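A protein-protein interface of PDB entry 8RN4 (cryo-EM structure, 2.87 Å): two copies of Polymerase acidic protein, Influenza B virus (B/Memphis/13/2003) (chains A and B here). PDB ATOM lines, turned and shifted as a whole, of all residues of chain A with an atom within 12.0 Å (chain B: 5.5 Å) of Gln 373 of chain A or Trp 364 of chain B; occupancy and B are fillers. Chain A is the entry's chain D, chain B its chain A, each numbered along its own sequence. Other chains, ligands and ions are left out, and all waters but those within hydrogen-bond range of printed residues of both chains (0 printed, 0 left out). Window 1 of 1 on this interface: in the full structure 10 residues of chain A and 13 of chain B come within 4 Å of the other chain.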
ATOM      1  N   LYS A 363     -19.408 -11.747 -31.221  1.00  0.00           N
ATOM      2  CA  LYS A 363     -19.623 -10.372 -30.785  1.00  0.00           C
ATOM      3  C   LYS A 363     -18.297  -9.661 -30.555  1.00  0.00           C
ATOM      4  O   LYS A 363     -18.143  -8.486 -30.909  1.00  0.00           O
ATOM      5  CB  LYS A 363     -20.468 -10.357 -29.510  1.00  0.00           C
ATOM      6  CG  LYS A 363     -20.756  -8.969 -28.960  1.00  0.00           C
ATOM      7  CD  LYS A 363     -21.463  -9.045 -27.617  1.00  0.00           C
ATOM      8  CE  LYS A 363     -21.238  -7.788 -26.797  1.00  0.00           C
ATOM      9  NZ  LYS A 363     -22.039  -7.791 -25.544  1.00  0.00           N
ATOM     10  N   TRP A 364     -17.329 -10.356 -29.962  1.00  0.00           N
ATOM     11  CA  TRP A 364     -16.028  -9.769 -29.670  1.00  0.00           C
ATOM     12  C   TRP A 364     -15.004 -10.035 -30.763  1.00  0.00           C
ATOM     13  O   TRP A 364     -14.111  -9.207 -30.978  1.00  0.00           O
ATOM     14  CB  TRP A 364     -15.504 -10.307 -28.337  1.00  0.00           C
ATOM     15  CG  TRP A 364     -16.408  -9.999 -27.189  1.00  0.00           C
ATOM     16  CD1 TRP A 364     -17.299 -10.844 -26.598  1.00  0.00           C
ATOM     17  CD2 TRP A 364     -16.514  -8.752 -26.494  1.00  0.00           C
ATOM     18  NE1 TRP A 364     -17.954 -10.201 -25.576  1.00  0.00           N
ATOM     19  CE2 TRP A 364     -17.489  -8.915 -25.492  1.00  0.00           C
ATOM     20  CE3 TRP A 364     -15.878  -7.515 -26.621  1.00  0.00           C
ATOM     21  CZ2 TRP A 364     -17.845  -7.887 -24.624  1.00  0.00           C
ATOM     22  CZ3 TRP A 364     -16.231  -6.496 -25.758  1.00  0.00           C
ATOM     23  CH2 TRP A 364     -17.205  -6.688 -24.772  1.00  0.00           C
ATOM     24  N   GLY A 367     -15.314  -7.403 -33.268  1.00  0.00           N
ATOM     25  CA  GLY A 367     -15.101  -6.078 -32.726  1.00  0.00           C
ATOM     26  C   GLY A 367     -16.359  -5.314 -32.376  1.00  0.00           C
ATOM     27  O   GLY A 367     -16.258  -4.168 -31.920  1.00  0.00           O
ATOM     28  N   ASP A 368     -17.541  -5.905 -32.571  1.00  0.00           N
ATOM     29  CA  ASP A 368     -18.775  -5.200 -32.240  1.00  0.00           C
ATOM     30  C   ASP A 368     -18.854  -4.881 -30.754  1.00  0.00           C
ATOM     31  O   ASP A 368     -19.483  -3.891 -30.364  1.00  0.00           O
ATOM     32  CB  ASP A 368     -19.986  -6.034 -32.663  1.00  0.00           C
ATOM     33  CG  ASP A 368     -20.420  -5.755 -34.091  1.00  0.00           C
ATOM     34  OD1 ASP A 368     -19.732  -4.979 -34.787  1.00  0.00           O
ATOM     35  OD2 ASP A 368     -21.451  -6.315 -34.517  1.00  0.00           O
ATOM     36  N   GLY A 369     -18.229  -5.704 -29.910  1.00  0.00           N
ATOM     37  CA  GLY A 369     -18.260  -5.442 -28.481  1.00  0.00           C
ATOM     38  C   GLY A 369     -17.516  -4.175 -28.101  1.00  0.00           C
ATOM     39  O   GLY A 369     -17.935  -3.446 -27.199  1.00  0.00           O
ATOM     40  N   LEU A 370     -16.404  -3.895 -28.784  1.00  0.00           N
ATOM     41  CA  LEU A 370     -15.584  -2.719 -28.490  1.00  0.00           C
ATOM     42  C   LEU A 370     -16.203  -1.490 -29.159  1.00  0.00           C
ATOM     43  O   LEU A 370     -15.708  -0.956 -30.153  1.00  0.00           O
ATOM     44  CB  LEU A 370     -14.150  -2.940 -28.949  1.00  0.00           C
ATOM     45  CG  LEU A 370     -13.393  -4.076 -28.262  1.00  0.00           C
ATOM     46  CD1 LEU A 370     -12.078  -4.338 -28.975  1.00  0.00           C
ATOM     47  CD2 LEU A 370     -13.158  -3.758 -26.795  1.00  0.00           C
ATOM     48  N   THR A 371     -17.316  -1.043 -28.585  1.00  0.00           N
ATOM     49  CA  THR A 371     -18.020   0.142 -29.050  1.00  0.00           C
ATOM     50  C   THR A 371     -18.315   1.046 -27.865  1.00  0.00           C
ATOM     51  O   THR A 371     -18.721   0.575 -26.798  1.00  0.00           O
ATOM     52  CB  THR A 371     -19.327  -0.223 -29.768  1.00  0.00           C
ATOM     53  OG1 THR A 371     -19.029  -0.906 -30.991  1.00  0.00           O
ATOM     54  CG2 THR A 371     -20.137   1.028 -30.075  1.00  0.00           C
ATOM     55  N   TYR A 372     -18.109   2.345 -28.057  1.00  0.00           N
ATOM     56  CA  TYR A 372     -18.346   3.308 -26.994  1.00  0.00           C
ATOM     57  C   TYR A 372     -19.834   3.386 -26.673  1.00  0.00           C
ATOM     58  O   TYR A 372     -20.691   3.097 -27.514  1.00  0.00           O
ATOM     59  CB  TYR A 372     -17.822   4.686 -27.397  1.00  0.00           C
ATOM     60  CG  TYR A 372     -16.316   4.762 -27.571  1.00  0.00           C
ATOM     61  CD1 TYR A 372     -15.515   3.638 -27.412  1.00  0.00           C
ATOM     62  CD2 TYR A 372     -15.699   5.960 -27.903  1.00  0.00           C
ATOM     63  CE1 TYR A 372     -14.146   3.707 -27.572  1.00  0.00           C
ATOM     64  CE2 TYR A 372     -14.329   6.037 -28.065  1.00  0.00           C
ATOM     65  CZ  TYR A 372     -13.559   4.907 -27.899  1.00  0.00           C
ATOM     66  OH  TYR A 372     -12.197   4.977 -28.060  1.00  0.00           O
ATOM     67  N   GLN A 373     -20.139   3.767 -25.436  1.00  0.00           N
ATOM     68  CA  GLN A 373     -21.511   3.893 -24.967  1.00  0.00           C
ATOM     69  C   GLN A 373     -21.859   5.367 -24.817  1.00  0.00           C
ATOM     70  O   GLN A 373     -21.100   6.131 -24.210  1.00  0.00           O
ATOM     71  CB  GLN A 373     -21.708   3.138 -23.647  1.00  0.00           C
ATOM     72  CG  GLN A 373     -21.577   3.964 -22.369  1.00  0.00           C
ATOM     73  CD  GLN A 373     -22.001   3.190 -21.137  1.00  0.00           C
ATOM     74  OE1 GLN A 373     -21.289   3.158 -20.135  1.00  0.00           O
ATOM     75  NE2 GLN A 373     -23.173   2.567 -21.200  1.00  0.00           N
ATOM     76  N   LYS A 374     -22.999   5.759 -25.377  1.00  0.00           N
ATOM     77  CA  LYS A 374     -23.419   7.151 -25.339  1.00  0.00           C
ATOM     78  C   LYS A 374     -23.838   7.553 -23.928  1.00  0.00           C
ATOM     79  O   LYS A 374     -24.371   6.749 -23.160  1.00  0.00           O
ATOM     80  CB  LYS A 374     -24.576   7.381 -26.310  1.00  0.00           C
ATOM     81  CG  LYS A 374     -24.513   8.699 -27.059  1.00  0.00           C
ATOM     82  CD  LYS A 374     -25.884   9.104 -27.579  1.00  0.00           C
ATOM     83  CE  LYS A 374     -25.780  10.025 -28.784  1.00  0.00           C
ATOM     84  NZ  LYS A 374     -25.242   9.323 -29.983  1.00  0.00           N
ATOM     85  N   ILE A 375     -23.587   8.819 -23.592  1.00  0.00           N
ATOM     86  CA  ILE A 375     -23.980   9.387 -22.311  1.00  0.00           C
ATOM     87  C   ILE A 375     -24.682  10.713 -22.568  1.00  0.00           C
ATOM     88  O   ILE A 375     -24.535  11.328 -23.627  1.00  0.00           O
ATOM     89  CB  ILE A 375     -22.776   9.584 -21.361  1.00  0.00           C
ATOM     90  CG1 ILE A 375     -21.867  10.708 -21.867  1.00  0.00           C
ATOM     91  CG2 ILE A 375     -21.997   8.286 -21.226  1.00  0.00           C
ATOM     92  CD1 ILE A 375     -20.546  10.804 -21.133  1.00  0.00           C
ATOM     93  N   MET A 376     -25.453  11.153 -21.578  1.00  0.00           N
ATOM     94  CA  MET A 376     -26.211  12.388 -21.728  1.00  0.00           C
ATOM     95  C   MET A 376     -25.262  13.576 -21.850  1.00  0.00           C
ATOM     96  O   MET A 376     -24.161  13.584 -21.293  1.00  0.00           O
ATOM     97  CB  MET A 376     -27.173  12.593 -20.552  1.00  0.00           C
ATOM     98  CG  MET A 376     -26.729  12.003 -19.221  1.00  0.00           C
ATOM     99  SD  MET A 376     -27.777  12.547 -17.859  1.00  0.00           S
ATOM    100  CE  MET A 376     -26.819  13.913 -17.212  1.00  0.00           C
ATOM    101  N   LYS A 377     -25.705  14.592 -22.594  1.00  0.00           N
ATOM    102  CA  LYS A 377     -24.821  15.699 -22.944  1.00  0.00           C
ATOM    103  C   LYS A 377     -24.339  16.462 -21.716  1.00  0.00           C
ATOM    104  O   LYS A 377     -23.250  17.045 -21.742  1.00  0.00           O
ATOM    105  CB  LYS A 377     -25.530  16.646 -23.915  1.00  0.00           C
ATOM    106  CG  LYS A 377     -26.689  17.436 -23.312  1.00  0.00           C
ATOM    107  CD  LYS A 377     -27.000  18.674 -24.136  1.00  0.00           C
ATOM    108  CE  LYS A 377     -28.402  19.190 -23.856  1.00  0.00           C
ATOM    109  NZ  LYS A 377     -29.421  18.541 -24.725  1.00  0.00           N
ATOM    110  N   GLU A 378     -25.128  16.482 -20.640  1.00  0.00           N
ATOM    111  CA  GLU A 378     -24.738  17.247 -19.459  1.00  0.00           C
ATOM    112  C   GLU A 378     -23.423  16.732 -18.887  1.00  0.00           C
ATOM    113  O   GLU A 378     -22.525  17.514 -18.551  1.00  0.00           O
ATOM    114  CB  GLU A 378     -25.845  17.184 -18.406  1.00  0.00           C
ATOM    115  CG  GLU A 378     -26.153  18.520 -17.751  1.00  0.00           C
ATOM    116  CD  GLU A 378     -26.976  18.375 -16.487  1.00  0.00           C
ATOM    117  OE1 GLU A 378     -27.834  17.470 -16.436  1.00  0.00           O
ATOM    118  OE2 GLU A 378     -26.764  19.166 -15.544  1.00  0.00           O
ATOM    119  N   VAL A 379     -23.287  15.408 -18.781  1.00  0.00           N
ATOM    120  CA  VAL A 379     -22.046  14.827 -18.279  1.00  0.00           C
ATOM    121  C   VAL A 379     -20.887  15.187 -19.196  1.00  0.00           C
ATOM    122  O   VAL A 379     -19.795  15.537 -18.733  1.00  0.00           O
ATOM    123  CB  VAL A 379     -22.198  13.301 -18.132  1.00  0.00           C
ATOM    124  CG1 VAL A 379     -20.896  12.677 -17.665  1.00  0.00           C
ATOM    125  CG2 VAL A 379     -23.321  12.974 -17.165  1.00  0.00           C
ATOM    126  N   ALA A 380     -21.105  15.110 -20.511  1.00  0.00           N
ATOM    127  CA  ALA A 380     -20.038  15.418 -21.457  1.00  0.00           C
ATOM    128  C   ALA A 380     -19.573  16.861 -21.314  1.00  0.00           C
ATOM    129  O   ALA A 380     -18.367  17.137 -21.330  1.00  0.00           O
ATOM    130  CB  ALA A 380     -20.514  15.146 -22.882  1.00  0.00           C
ATOM    131  N   ILE A 381     -20.512  17.799 -21.174  1.00  0.00           N
ATOM    132  CA  ILE A 381     -20.137  19.195 -20.964  1.00  0.00           C
ATOM    133  C   ILE A 381     -19.358  19.337 -19.664  1.00  0.00           C
ATOM    134  O   ILE A 381     -18.322  20.010 -19.608  1.00  0.00           O
ATOM    135  CB  ILE A 381     -21.383  20.101 -20.974  1.00  0.00           C
ATOM    136  CG1 ILE A 381     -22.141  19.995 -22.303  1.00  0.00           C
ATOM    137  CG2 ILE A 381     -20.990  21.548 -20.710  1.00  0.00           C
ATOM    138  CD1 ILE A 381     -21.259  19.931 -23.532  1.00  0.00           C
ATOM    139  N   ASP A 382     -19.846  18.705 -18.594  1.00  0.00           N
ATOM    140  CA  ASP A 382     -19.137  18.776 -17.321  1.00  0.00           C
ATOM    141  C   ASP A 382     -17.795  18.056 -17.396  1.00  0.00           C
ATOM    142  O   ASP A 382     -16.797  18.535 -16.844  1.00  0.00           O
ATOM    143  CB  ASP A 382     -20.001  18.189 -16.207  1.00  0.00           C
ATOM    144  CG  ASP A 382     -21.082  19.147 -15.746  1.00  0.00           C
ATOM    145  OD1 ASP A 382     -21.016  20.342 -16.101  1.00  0.00           O
ATOM    146  OD2 ASP A 382     -22.002  18.704 -15.027  1.00  0.00           O
ATOM    147  N   ASP A 383     -17.748  16.911 -18.071  1.00  0.00           N
ATOM    148  CA  ASP A 383     -16.502  16.169 -18.200  1.00  0.00           C
ATOM    149  C   ASP A 383     -15.532  16.924 -19.103  1.00  0.00           C
ATOM    150  O   ASP A 383     -15.906  17.389 -20.184  1.00  0.00           O
ATOM    151  CB  ASP A 383     -16.774  14.775 -18.762  1.00  0.00           C
ATOM    152  CG  ASP A 383     -15.596  13.835 -18.589  1.00  0.00           C
ATOM    153  OD1 ASP A 383     -14.456  14.322 -18.449  1.00  0.00           O
ATOM    154  OD2 ASP A 383     -15.812  12.605 -18.597  1.00  0.00           O
ATOM    155  N   GLU A 384     -14.282  17.043 -18.655  1.00  0.00           N
ATOM    156  CA  GLU A 384     -13.258  17.748 -19.416  1.00  0.00           C
ATOM    157  C   GLU A 384     -12.406  16.811 -20.262  1.00  0.00           C
ATOM    158  O   GLU A 384     -11.870  17.235 -21.292  1.00  0.00           O
ATOM    159  CB  GLU A 384     -12.357  18.543 -18.463  1.00  0.00           C
ATOM    160  CG  GLU A 384     -10.910  18.688 -18.920  1.00  0.00           C
ATOM    161  CD  GLU A 384     -10.125  19.662 -18.064  1.00  0.00           C
ATOM    162  OE1 GLU A 384     -10.179  19.540 -16.822  1.00  0.00           O
ATOM    163  OE2 GLU A 384      -9.453  20.548 -18.632  1.00  0.00           O
ATOM    164  N   THR A 385     -12.271  15.547 -19.851  1.00  0.00           N
ATOM    165  CA  THR A 385     -11.411  14.619 -20.578  1.00  0.00           C
ATOM    166  C   THR A 385     -11.927  14.354 -21.987  1.00  0.00           C
ATOM    167  O   THR A 385     -11.142  14.007 -22.876  1.00  0.00           O
ATOM    168  CB  THR A 385     -11.293  13.305 -19.804  1.00  0.00           C
ATOM    169  OG1 THR A 385     -10.449  13.496 -18.662  1.00  0.00           O
ATOM    170  CG2 THR A 385     -10.709  12.203 -20.683  1.00  0.00           C
ATOM    171  N   MET A 386     -13.229  14.515 -22.214  1.00  0.00           N
ATOM    172  CA  MET A 386     -13.826  14.207 -23.509  1.00  0.00           C
ATOM    173  C   MET A 386     -13.614  15.387 -24.449  1.00  0.00           C
ATOM    174  O   MET A 386     -14.102  16.492 -24.193  1.00  0.00           O
ATOM    175  CB  MET A 386     -15.312  13.891 -23.352  1.00  0.00           C
ATOM    176  CG  MET A 386     -15.658  13.129 -22.078  1.00  0.00           C
ATOM    177  SD  MET A 386     -16.930  11.875 -22.324  1.00  0.00           S
ATOM    178  CE  MET A 386     -18.120  12.780 -23.306  1.00  0.00           C
ATOM    179  N   GLU A 389     -12.475  14.195 -31.447  1.00  0.00           N
ATOM    180  CA  GLU A 389     -11.417  13.425 -32.086  1.00  0.00           C
ATOM    181  C   GLU A 389     -10.996  14.085 -33.392  1.00  0.00           C
ATOM    182  O   GLU A 389     -11.823  14.630 -34.128  1.00  0.00           O
ATOM    183  CB  GLU A 389     -11.882  11.991 -32.347  1.00  0.00           C
ATOM    184  CG  GLU A 389     -13.185  11.884 -33.127  1.00  0.00           C
ATOM    185  CD  GLU A 389     -14.385  11.673 -32.227  1.00  0.00           C
ATOM    186  OE1 GLU A 389     -14.661  12.556 -31.389  1.00  0.00           O
ATOM    187  OE2 GLU A 389     -15.052  10.625 -32.359  1.00  0.00           O
ATOM    188  N   PHE B 335     -18.663  17.447 -11.425  1.00  0.00           N
ATOM    189  CA  PHE B 335     -19.410  16.291 -10.939  1.00  0.00           C
ATOM    190  C   PHE B 335     -19.734  16.437  -9.459  1.00  0.00           C
ATOM    191  O   PHE B 335     -20.884  16.267  -9.042  1.00  0.00           O
ATOM    192  CB  PHE B 335     -18.613  15.007 -11.173  1.00  0.00           C
ATOM    193  CG  PHE B 335     -18.578  14.546 -12.607  1.00  0.00           C
ATOM    194  CD1 PHE B 335     -19.246  15.235 -13.605  1.00  0.00           C
ATOM    195  CD2 PHE B 335     -17.871  13.407 -12.951  1.00  0.00           C
ATOM    196  CE1 PHE B 335     -19.204  14.798 -14.913  1.00  0.00           C
ATOM    197  CE2 PHE B 335     -17.827  12.968 -14.255  1.00  0.00           C
ATOM    198  CZ  PHE B 335     -18.493  13.663 -15.236  1.00  0.00           C
ATOM    199  N   ASN B 360     -29.086   9.661 -13.134  1.00  0.00           N
ATOM    200  CA  ASN B 360     -28.345   9.406 -14.365  1.00  0.00           C
ATOM    201  C   ASN B 360     -27.072  10.229 -14.442  1.00  0.00           C
ATOM    202  O   ASN B 360     -26.038   9.718 -14.880  1.00  0.00           O
ATOM    203  CB  ASN B 360     -29.231   9.696 -15.585  1.00  0.00           C
ATOM    204  CG  ASN B 360     -29.740   8.432 -16.249  1.00  0.00           C
ATOM    205  OD1 ASN B 360     -29.011   7.450 -16.384  1.00  0.00           O
ATOM    206  ND2 ASN B 360     -31.001   8.449 -16.662  1.00  0.00           N
ATOM    207  N   TYR B 361     -27.122  11.496 -14.029  1.00  0.00           N
ATOM    208  CA  TYR B 361     -25.897  12.252 -13.815  1.00  0.00           C
ATOM    209  C   TYR B 361     -25.096  11.661 -12.662  1.00  0.00           C
ATOM    210  O   TYR B 361     -23.862  11.599 -12.720  1.00  0.00           O
ATOM    211  CB  TYR B 361     -26.230  13.718 -13.547  1.00  0.00           C
ATOM    212  CG  TYR B 361     -25.026  14.624 -13.542  1.00  0.00           C
ATOM    213  CD1 TYR B 361     -24.264  14.789 -12.395  1.00  0.00           C
ATOM    214  CD2 TYR B 361     -24.649  15.316 -14.682  1.00  0.00           C
ATOM    215  CE1 TYR B 361     -23.163  15.614 -12.384  1.00  0.00           C
ATOM    216  CE2 TYR B 361     -23.548  16.144 -14.681  1.00  0.00           C
ATOM    217  CZ  TYR B 361     -22.810  16.288 -13.529  1.00  0.00           C
ATOM    218  OH  TYR B 361     -21.713  17.113 -13.520  1.00  0.00           O
ATOM    219  N   ALA B 362     -25.784  11.223 -11.605  1.00  0.00           N
ATOM    220  CA  ALA B 362     -25.112  10.599 -10.473  1.00  0.00           C
ATOM    221  C   ALA B 362     -24.473   9.268 -10.845  1.00  0.00           C
ATOM    222  O   ALA B 362     -23.567   8.813 -10.140  1.00  0.00           O
ATOM    223  CB  ALA B 362     -26.101  10.393  -9.326  1.00  0.00           C
ATOM    224  N   LYS B 363     -24.924   8.634 -11.929  1.00  0.00           N
ATOM    225  CA  LYS B 363     -24.295   7.394 -12.368  1.00  0.00           C
ATOM    226  C   LYS B 363     -22.849   7.626 -12.779  1.00  0.00           C
ATOM    227  O   LYS B 363     -22.008   6.732 -12.627  1.00  0.00           O
ATOM    228  CB  LYS B 363     -25.088   6.789 -13.526  1.00  0.00           C
ATOM    229  CG  LYS B 363     -24.589   5.431 -13.997  1.00  0.00           C
ATOM    230  CD  LYS B 363     -25.030   5.148 -15.423  1.00  0.00           C
ATOM    231  CE  LYS B 363     -25.136   3.656 -15.692  1.00  0.00           C
ATOM    232  NZ  LYS B 363     -23.800   3.024 -15.870  1.00  0.00           N
ATOM    233  N   TRP B 364     -22.541   8.812 -13.301  1.00  0.00           N
ATOM    234  CA  TRP B 364     -21.186   9.167 -13.700  1.00  0.00           C
ATOM    235  C   TRP B 364     -20.494  10.085 -12.707  1.00  0.00           C
ATOM    236  O   TRP B 364     -19.264  10.047 -12.601  1.00  0.00           O
ATOM    237  CB  TRP B 364     -21.206   9.840 -15.076  1.00  0.00           C
ATOM    238  CG  TRP B 364     -21.905   9.022 -16.109  1.00  0.00           C
ATOM    239  CD1 TRP B 364     -23.170   9.204 -16.583  1.00  0.00           C
ATOM    240  CD2 TRP B 364     -21.377   7.884 -16.797  1.00  0.00           C
ATOM    241  NE1 TRP B 364     -23.464   8.247 -17.524  1.00  0.00           N
ATOM    242  CE2 TRP B 364     -22.378   7.425 -17.673  1.00  0.00           C
ATOM    243  CE3 TRP B 364     -20.155   7.208 -16.756  1.00  0.00           C
ATOM    244  CZ2 TRP B 364     -22.195   6.324 -18.501  1.00  0.00           C
ATOM    245  CZ3 TRP B 364     -19.976   6.116 -17.579  1.00  0.00           C
ATOM    246  CH2 TRP B 364     -20.989   5.685 -18.440  1.00  0.00           C
ATOM    247  N   ALA B 365     -21.250  10.907 -11.977  1.00  0.00           N
ATOM    248  CA  ALA B 365     -20.640  11.764 -10.968  1.00  0.00           C
ATOM    249  C   ALA B 365     -19.981  10.934  -9.875  1.00  0.00           C
ATOM    250  O   ALA B 365     -18.900  11.283  -9.386  1.00  0.00           O
ATOM    251  CB  ALA B 365     -21.691  12.700 -10.374  1.00  0.00           C
ATOM    252  N   THR B 366     -20.618   9.834  -9.478  1.00  0.00           N
ATOM    253  CA  THR B 366     -20.060   8.944  -8.469  1.00  0.00           C
ATOM    254  C   THR B 366     -19.051   7.959  -9.042  1.00  0.00           C
ATOM    255  O   THR B 366     -18.434   7.216  -8.273  1.00  0.00           O
ATOM    256  CB  THR B 366     -21.181   8.167  -7.776  1.00  0.00           C
ATOM    257  OG1 THR B 366     -21.796   7.274  -8.712  1.00  0.00           O
ATOM    258  CG2 THR B 366     -22.231   9.116  -7.224  1.00  0.00           C
ATOM    259  N   GLY B 367     -18.869   7.931 -10.359  1.00  0.00           N
ATOM    260  CA  GLY B 367     -17.937   7.009 -10.975  1.00  0.00           C
ATOM    261  C   GLY B 367     -18.447   5.597 -11.130  1.00  0.00           C
ATOM    262  O   GLY B 367     -17.668   4.712 -11.501  1.00  0.00           O
ATOM    263  N   ASP B 368     -19.731   5.353 -10.858  1.00  0.00           N
ATOM    264  CA  ASP B 368     -20.269   4.002 -10.985  1.00  0.00           C
ATOM    265  C   ASP B 368     -20.244   3.527 -12.431  1.00  0.00           C
ATOM    266  O   ASP B 368     -19.956   2.354 -12.700  1.00  0.00           O
ATOM    267  CB  ASP B 368     -21.693   3.954 -10.431  1.00  0.00           C
ATOM    268  CG  ASP B 368     -21.729   3.917  -8.918  1.00  0.00           C
ATOM    269  OD1 ASP B 368     -20.648   3.870  -8.295  1.00  0.00           O
ATOM    270  OD2 ASP B 368     -22.840   3.931  -8.348  1.00  0.00           O
ATOM    271  N   GLY B 369     -20.543   4.418 -13.378  1.00  0.00           N
ATOM    272  CA  GLY B 369     -20.601   4.026 -14.774  1.00  0.00           C
ATOM    273  C   GLY B 369     -19.264   3.628 -15.363  1.00  0.00           C
ATOM    274  O   GLY B 369     -19.232   2.981 -16.414  1.00  0.00           O
ATOM    275  N   LEU B 370     -18.163   3.999 -14.714  1.00  0.00           N
ATOM    276  CA  LEU B 370     -16.823   3.670 -15.202  1.00  0.00           C
ATOM    277  C   LEU B 370     -16.357   2.335 -14.622  1.00  0.00           C
ATOM    278  O   LEU B 370     -15.320   2.227 -13.967  1.00  0.00           O
ATOM    279  CB  LEU B 370     -15.850   4.791 -14.858  1.00  0.00           C
ATOM    280  CG  LEU B 370     -16.013   6.114 -15.609  1.00  0.00           C
ATOM    281  CD1 LEU B 370     -14.895   7.067 -15.231  1.00  0.00           C
ATOM    282  CD2 LEU B 370     -16.040   5.899 -17.112  1.00  0.00           C
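OH of Tyr 361 of chain B sits close to OD2 of Asp 382 of chain A.
Among the printed residues, merely in contact across the chains: Gln 373 of chain A with Trp 364 of chain B, Ile 375 of chain A with Trp 364 of chain B, Val 379 of chain A with Phe 335 of chain B, Met 376 of chain A with Tyr 361 of chain B, Val 379 of chain A with Tyr 361 of chain B, Asp 382 of chain A with Phe 335 of chain B, Val 379 of chain A with Trp 364 of chain B and Met 376 of chain A with Asn 360 of chain B.
Of chain A, only Gln 373, Ile 375 and Val 379 come within 4 Å of Trp 364 of chain B. Phe 335 of chain B touches just these residues of chain A: Val 379 and Asp 382. Asn 360 of chain B touches just one residue of chain A: Met 376. Tyr 361 of chain B touches just these residues of chain A: Met 376 (3.6 Å), Val 379 (3.7 Å) and Asp 382 (2.2 Å). No residue of chain A comes within 4 Å of Gly 367 of chain B. No residue of chain A comes within 4 Å of Asp 368 of chain B. No residue of chain A comes within 4 Å of Leu 370 of chain B. Of the printed residues of chain B, Asp 382 of chain A touches Phe 335 (3.7 Å) and Tyr 361 (2.2 Å). Printed residues of chain B within 4 Å of Met 376 of chain A: Asn 360 (3.9 Å) and Tyr 361 (3.6 Å). Lys 363 of chain A touches none of the printed residues of chain B. Thr 371 of chain A touches none of the printed residues of chain B. The nearest residue of chain B that does not touch Gln 373 of chain A is Gly 369 of chain B (4.3 Å).
Printed residues of chain B that touch a printed residue of chain A: Phe 335, Asn 360, Tyr 361 and Trp 364. Hydrophobic or aromatic side chains of chain B within 4 Å of the printed part of chain A: Phe 335, Tyr 361 and Trp 364. Among the printed residues, no Asp or Glu carboxylate lies within 4 Å of a Lys or Arg side-chain nitrogen of the other chain.
Positions printed for both chains: 363, 364, 367, 368, 369 and 370. Of the 9 pairs that touch across the chains among the printed residues, none has its exchanged pair printed and touching as well.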
